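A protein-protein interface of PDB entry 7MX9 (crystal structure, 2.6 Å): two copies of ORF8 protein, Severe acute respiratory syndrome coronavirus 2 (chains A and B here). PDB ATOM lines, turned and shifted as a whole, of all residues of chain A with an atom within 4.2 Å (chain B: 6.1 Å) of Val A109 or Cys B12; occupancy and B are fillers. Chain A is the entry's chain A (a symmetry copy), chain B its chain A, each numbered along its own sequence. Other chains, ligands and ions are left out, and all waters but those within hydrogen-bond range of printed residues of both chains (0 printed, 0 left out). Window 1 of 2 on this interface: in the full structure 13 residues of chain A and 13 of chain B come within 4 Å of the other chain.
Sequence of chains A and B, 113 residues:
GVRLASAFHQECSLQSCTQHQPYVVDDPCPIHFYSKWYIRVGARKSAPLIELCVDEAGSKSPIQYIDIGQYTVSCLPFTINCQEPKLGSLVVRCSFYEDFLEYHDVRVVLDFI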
ATOM      1  N   CYS A  12     -16.476 -16.840 -30.404  1.00  0.00           N
ATOM      2  CA  CYS A  12     -16.481 -15.774 -29.415  1.00  0.00           C
ATOM      3  C   CYS A  12     -15.439 -16.083 -28.352  1.00  0.00           C
ATOM      4  O   CYS A  12     -15.144 -17.248 -28.073  1.00  0.00           O
ATOM      5  CB  CYS A  12     -17.871 -15.620 -28.787  1.00  0.00           C
ATOM      6  SG  CYS A  12     -18.010 -14.317 -27.555  1.00  0.00           S
ATOM      7  N   SER A  13     -14.885 -15.025 -27.759  1.00  0.00           N
ATOM      8  CA  SER A  13     -13.830 -15.148 -26.759  1.00  0.00           C
ATOM      9  C   SER A  13     -14.156 -14.266 -25.564  1.00  0.00           C
ATOM     10  O   SER A  13     -14.346 -13.055 -25.715  1.00  0.00           O
ATOM     11  CB  SER A  13     -12.472 -14.758 -27.346  1.00  0.00           C
ATOM     12  OG  SER A  13     -11.429 -15.009 -26.420  1.00  0.00           O
ATOM     13  N   LEU A  14     -14.205 -14.873 -24.381  1.00  0.00           N
ATOM     14  CA  LEU A  14     -14.443 -14.162 -23.132  1.00  0.00           C
ATOM     15  C   LEU A  14     -13.118 -14.022 -22.392  1.00  0.00           C
ATOM     16  O   LEU A  14     -12.504 -15.026 -22.017  1.00  0.00           O
ATOM     17  CB  LEU A  14     -15.466 -14.903 -22.272  1.00  0.00           C
ATOM     18  CG  LEU A  14     -15.788 -14.285 -20.908  1.00  0.00           C
ATOM     19  CD1 LEU A  14     -16.403 -12.905 -21.069  1.00  0.00           C
ATOM     20  CD2 LEU A  14     -16.716 -15.197 -20.114  1.00  0.00           C
ATOM     21  N   GLN A  15     -12.685 -12.783 -22.184  1.00  0.00           N
ATOM     22  CA  GLN A  15     -11.413 -12.486 -21.541  1.00  0.00           C
ATOM     23  C   GLN A  15     -11.652 -11.633 -20.306  1.00  0.00           C
ATOM     24  O   GLN A  15     -12.517 -10.751 -20.306  1.00  0.00           O
ATOM     25  CB  GLN A  15     -10.467 -11.760 -22.502  1.00  0.00           C
ATOM     26  CG  GLN A  15     -10.350 -12.407 -23.873  1.00  0.00           C
ATOM     27  CD  GLN A  15      -8.957 -12.289 -24.461  1.00  0.00           C
ATOM     28  OE1 GLN A  15      -8.098 -11.589 -23.924  1.00  0.00           O
ATOM     29  NE2 GLN A  15      -8.729 -12.972 -25.577  1.00  0.00           N
ATOM     30  N   GLU A  84     -14.766  -1.782 -22.730  1.00  0.00           N
ATOM     31  CA  GLU A  84     -15.480  -1.946 -23.992  1.00  0.00           C
ATOM     32  C   GLU A  84     -15.397  -0.662 -24.816  1.00  0.00           C
ATOM     33  O   GLU A  84     -15.664   0.422 -24.290  1.00  0.00           O
ATOM     34  CB  GLU A  84     -16.950  -2.296 -23.751  1.00  0.00           C
ATOM     35  CG  GLU A  84     -17.226  -3.768 -23.527  1.00  0.00           C
ATOM     36  CD  GLU A  84     -16.974  -4.604 -24.763  1.00  0.00           C
ATOM     37  OE1 GLU A  84     -17.298  -4.135 -25.876  1.00  0.00           O
ATOM     38  OE2 GLU A  84     -16.460  -5.733 -24.622  1.00  0.00           O
ATOM     39  N   ARG A 107     -15.333 -12.561 -31.948  1.00  0.00           N
ATOM     40  CA  ARG A 107     -15.627 -11.407 -31.114  1.00  0.00           C
ATOM     41  C   ARG A 107     -14.953 -11.560 -29.758  1.00  0.00           C
ATOM     42  O   ARG A 107     -14.904 -12.656 -29.193  1.00  0.00           O
ATOM     43  CB  ARG A 107     -17.131 -11.224 -30.923  1.00  0.00           C
ATOM     44  CG  ARG A 107     -17.466  -9.954 -30.140  1.00  0.00           C
ATOM     45  CD  ARG A 107     -18.915  -9.516 -30.299  1.00  0.00           C
ATOM     46  NE  ARG A 107     -19.413  -9.687 -31.661  1.00  0.00           N
ATOM     47  CZ  ARG A 107     -20.635  -9.350 -32.058  1.00  0.00           C
ATOM     48  NH1 ARG A 107     -21.491  -8.812 -31.197  1.00  0.00           N
ATOM     49  NH2 ARG A 107     -21.003  -9.547 -33.315  1.00  0.00           N
ATOM     50  N   VAL A 108     -14.432 -10.453 -29.239  1.00  0.00           N
ATOM     51  CA  VAL A 108     -13.749 -10.425 -27.952  1.00  0.00           C
ATOM     52  C   VAL A 108     -14.603  -9.616 -26.990  1.00  0.00           C
ATOM     53  O   VAL A 108     -14.824  -8.414 -27.200  1.00  0.00           O
ATOM     54  CB  VAL A 108     -12.334  -9.841 -28.066  1.00  0.00           C
ATOM     55  CG1 VAL A 108     -11.803  -9.481 -26.687  1.00  0.00           C
ATOM     56  CG2 VAL A 108     -11.404 -10.840 -28.745  1.00  0.00           C
ATOM     57  N   VAL A 109     -15.095 -10.278 -25.949  1.00  0.00           N
ATOM     58  CA  VAL A 109     -15.941  -9.671 -24.936  1.00  0.00           C
ATOM     59  C   VAL A 109     -15.224  -9.772 -23.595  1.00  0.00           C
ATOM     60  O   VAL A 109     -14.690 -10.833 -23.244  1.00  0.00           O
ATOM     61  CB  VAL A 109     -17.318 -10.353 -24.885  1.00  0.00           C
ATOM     62  CG1 VAL A 109     -17.155 -11.862 -24.735  1.00  0.00           C
ATOM     63  CG2 VAL A 109     -18.138  -9.794 -23.712  1.00  0.00           C
ATOM     64  N   LEU A 110     -15.224  -8.678 -22.845  1.00  0.00           N
ATOM     65  CA  LEU A 110     -14.505  -8.583 -21.587  1.00  0.00           C
ATOM     66  C   LEU A 110     -15.468  -8.603 -20.406  1.00  0.00           C
ATOM     67  O   LEU A 110     -16.611  -8.146 -20.505  1.00  0.00           O
ATOM     68  CB  LEU A 110     -13.685  -7.290 -21.529  1.00  0.00           C
ATOM     69  CG  LEU A 110     -12.798  -6.874 -22.702  1.00  0.00           C
ATOM     70  CD1 LEU A 110     -12.329  -5.435 -22.510  1.00  0.00           C
ATOM     71  CD2 LEU A 110     -11.617  -7.810 -22.816  1.00  0.00           C
ATOM     72  N   GLU B  11     -15.791 -19.507 -21.282  1.00  0.00           N
ATOM     73  CA  GLU B  11     -16.267 -19.762 -22.638  1.00  0.00           C
ATOM     74  C   GLU B  11     -17.357 -18.771 -23.026  1.00  0.00           C
ATOM     75  O   GLU B  11     -17.941 -18.107 -22.168  1.00  0.00           O
ATOM     76  CB  GLU B  11     -16.783 -21.194 -22.761  1.00  0.00           C
ATOM     77  CG  GLU B  11     -15.684 -22.242 -22.743  1.00  0.00           C
ATOM     78  CD  GLU B  11     -16.202 -23.633 -23.050  1.00  0.00           C
ATOM     79  OE1 GLU B  11     -17.406 -23.766 -23.357  1.00  0.00           O
ATOM     80  OE2 GLU B  11     -15.404 -24.592 -22.986  1.00  0.00           O
ATOM     81  N   CYS B  12     -17.631 -18.680 -24.325  1.00  0.00           N
ATOM     82  CA  CYS B  12     -18.526 -17.663 -24.855  1.00  0.00           C
ATOM     83  C   CYS B  12     -19.201 -18.203 -26.105  1.00  0.00           C
ATOM     84  O   CYS B  12     -18.635 -19.031 -26.824  1.00  0.00           O
ATOM     85  CB  CYS B  12     -17.759 -16.371 -25.164  1.00  0.00           C
ATOM     86  SG  CYS B  12     -18.763 -15.027 -25.812  1.00  0.00           S
ATOM     87  N   SER B  13     -20.418 -17.723 -26.359  1.00  0.00           N
ATOM     88  CA  SER B  13     -21.223 -18.179 -27.487  1.00  0.00           C
ATOM     89  C   SER B  13     -21.796 -16.978 -28.222  1.00  0.00           C
ATOM     90  O   SER B  13     -22.487 -16.149 -27.621  1.00  0.00           O
ATOM     91  CB  SER B  13     -22.354 -19.097 -27.016  1.00  0.00           C
ATOM     92  OG  SER B  13     -23.049 -19.650 -28.120  1.00  0.00           O
ATOM     93  N   LEU B  14     -21.521 -16.898 -29.521  1.00  0.00           N
ATOM     94  CA  LEU B  14     -22.044 -15.844 -30.381  1.00  0.00           C
ATOM     95  C   LEU B  14     -23.182 -16.419 -31.217  1.00  0.00           C
ATOM     96  O   LEU B  14     -22.966 -17.336 -32.015  1.00  0.00           O
ATOM     97  CB  LEU B  14     -20.945 -15.280 -31.280  1.00  0.00           C
ATOM     98  CG  LEU B  14     -21.362 -14.185 -32.266  1.00  0.00           C
ATOM     99  CD1 LEU B  14     -21.873 -12.958 -31.529  1.00  0.00           C
ATOM    100  CD2 LEU B  14     -20.199 -13.818 -33.180  1.00  0.00           C
ATOM    101  N   ASP B 105     -19.632 -21.933 -16.934  1.00  0.00           N
ATOM    102  CA  ASP B 105     -20.558 -20.923 -17.424  1.00  0.00           C
ATOM    103  C   ASP B 105     -20.174 -20.531 -18.842  1.00  0.00           C
ATOM    104  O   ASP B 105     -19.005 -20.591 -19.228  1.00  0.00           O
ATOM    105  CB  ASP B 105     -20.569 -19.685 -16.525  1.00  0.00           C
ATOM    106  CG  ASP B 105     -21.185 -19.953 -15.160  1.00  0.00           C
ATOM    107  OD1 ASP B 105     -21.736 -21.053 -14.958  1.00  0.00           O
ATOM    108  OD2 ASP B 105     -21.118 -19.055 -14.291  1.00  0.00           O
ATOM    109  N   VAL B 106     -21.179 -20.143 -19.621  1.00  0.00           N
ATOM    110  CA  VAL B 106     -20.987 -19.743 -21.010  1.00  0.00           C
ATOM    111  C   VAL B 106     -21.827 -18.506 -21.260  1.00  0.00           C
ATOM    112  O   VAL B 106     -23.063 -18.565 -21.180  1.00  0.00           O
ATOM    113  CB  VAL B 106     -21.375 -20.860 -21.995  1.00  0.00           C
ATOM    114  CG1 VAL B 106     -21.184 -20.391 -23.430  1.00  0.00           C
ATOM    115  CG2 VAL B 106     -20.567 -22.117 -21.722  1.00  0.00           C
ATOM    116  N   ARG B 107     -21.182 -17.380 -21.550  1.00  0.00           N
ATOM    117  CA  ARG B 107     -21.912 -16.162 -21.861  1.00  0.00           C
ATOM    118  C   ARG B 107     -22.485 -16.244 -23.269  1.00  0.00           C
ATOM    119  O   ARG B 107     -21.840 -16.755 -24.188  1.00  0.00           O
ATOM    120  CB  ARG B 107     -21.020 -14.929 -21.740  1.00  0.00           C
ATOM    121  CG  ARG B 107     -21.795 -13.629 -21.955  1.00  0.00           C
ATOM    122  CD  ARG B 107     -21.065 -12.401 -21.429  1.00  0.00           C
ATOM    123  NE  ARG B 107     -20.387 -12.646 -20.158  1.00  0.00           N
ATOM    124  CZ  ARG B 107     -19.708 -11.725 -19.484  1.00  0.00           C
ATOM    125  NH1 ARG B 107     -19.620 -10.486 -19.953  1.00  0.00           N
ATOM    126  NH2 ARG B 107     -19.119 -12.039 -18.339  1.00  0.00           N
ATOM    127  N   VAL B 108     -23.702 -15.737 -23.432  1.00  0.00           N
ATOM    128  CA  VAL B 108     -24.398 -15.737 -24.712  1.00  0.00           C
ATOM    129  C   VAL B 108     -24.515 -14.295 -25.177  1.00  0.00           C
ATOM    130  O   VAL B 108     -25.169 -13.472 -24.521  1.00  0.00           O
ATOM    131  CB  VAL B 108     -25.776 -16.406 -24.617  1.00  0.00           C
ATOM    132  CG1 VAL B 108     -26.612 -16.061 -25.841  1.00  0.00           C
ATOM    133  CG2 VAL B 108     -25.623 -17.917 -24.492  1.00  0.00           C
ATOM    134  N   VAL B 109     -23.869 -13.990 -26.297  1.00  0.00           N
ATOM    135  CA  VAL B 109     -23.860 -12.660 -26.883  1.00  0.00           C
ATOM    136  C   VAL B 109     -24.497 -12.744 -28.265  1.00  0.00           C
ATOM    137  O   VAL B 109     -24.181 -13.650 -29.050  1.00  0.00           O
ATOM    138  CB  VAL B 109     -22.429 -12.102 -26.961  1.00  0.00           C
ATOM    139  CG1 VAL B 109     -21.511 -13.097 -27.664  1.00  0.00           C
ATOM    140  CG2 VAL B 109     -22.428 -10.762 -27.716  1.00  0.00           C
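The side-chain sulfur (SG) of Cys B12 forms a disulfide with the side-chain sulfur (SG) of Cys A12, 2.0 Å away.
Printed residues of chain B that touch a printed residue of chain A: Glu B11, Cys B12, Leu B14, Arg B107 and Val B109. Hydrophobic or aromatic side chains of chain B within 4 Å of the printed part of chain A: Leu B14 and Val B109. Of the 9 printed residues of chain A, 5 touch a printed residue of chain B. Hydrophobic or aromatic side chains of chain A within 4 Å of the printed part of chain B: Leu A14 and Val A109. Among the printed residues, 9 pairs touch across the chains.
Cys B12 touches its own counterpart, Cys A12. Cys A12 touches Leu B14, and with the chains exchanged Leu A14 touches Cys B12. Cys A12 touches Val B109, and with the chains exchanged Val A109 touches Cys B12. Leu A14 touches Arg B107, and with the chains exchanged Arg A107 touches Leu B14. 6 positions are printed for both chains. Of the 9 pairs that touch across the chains among the printed residues, 7 have their exchanged pair printed and touching as well.
Of the printed residues of chain B, Cys A12 touches Cys B12, Leu B14 and Val B109. Of the printed residues of chain B, Leu A14 touches Glu B11, Cys B12 and Arg B107. Of the printed residues of chain B, Arg A107 touches Leu B14 (3.9 Å). Printed residues of chain B within 4 Å of Val A109: Cys B12. Of the printed residues of chain A, Glu B11 touches Leu A14. Cys B12 touches three residues of chain A. Printed residues of chain A within 4 Å of Val B109: Cys A12 (3.7 Å).
O of Glu B11 sits at hydrogen-bond distance from N of Arg B107 (3.4 Å). The backbone carbonyl oxygen (O) of Ser A13 is in hydrogen-bond range of the backbone NH (N) of Val A109, 2.9 Å away. O of Arg B107 sits at hydrogen-bond distance from N of Ser B13, 2.8 Å away. N of Val B109 sits at hydrogen-bond distance from O of Ser B13 (2.9 Å). N of Gln A15 is in hydrogen-bond range of O of Val A109, at 3.0 Å. The backbone NH (N) of Ser A13 lies within hydrogen-bond range of the backbone carbonyl oxygen (O) of Arg A107 (2.8 Å).
Cys A12 touches Leu B14. Cys A12 touches Val B109 (SG to CG1, 3.7 Å). Glu B11 touches Leu A14. Leu A14 touches Cys B12. Leu A14 touches Arg B107. CD1 of Leu B14 touches CZ of Arg A107 (3.9 Å). SG of Cys B12 touches CG1 of Val A109, 3.7 Å away. Arg B107 touches Leu A110.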
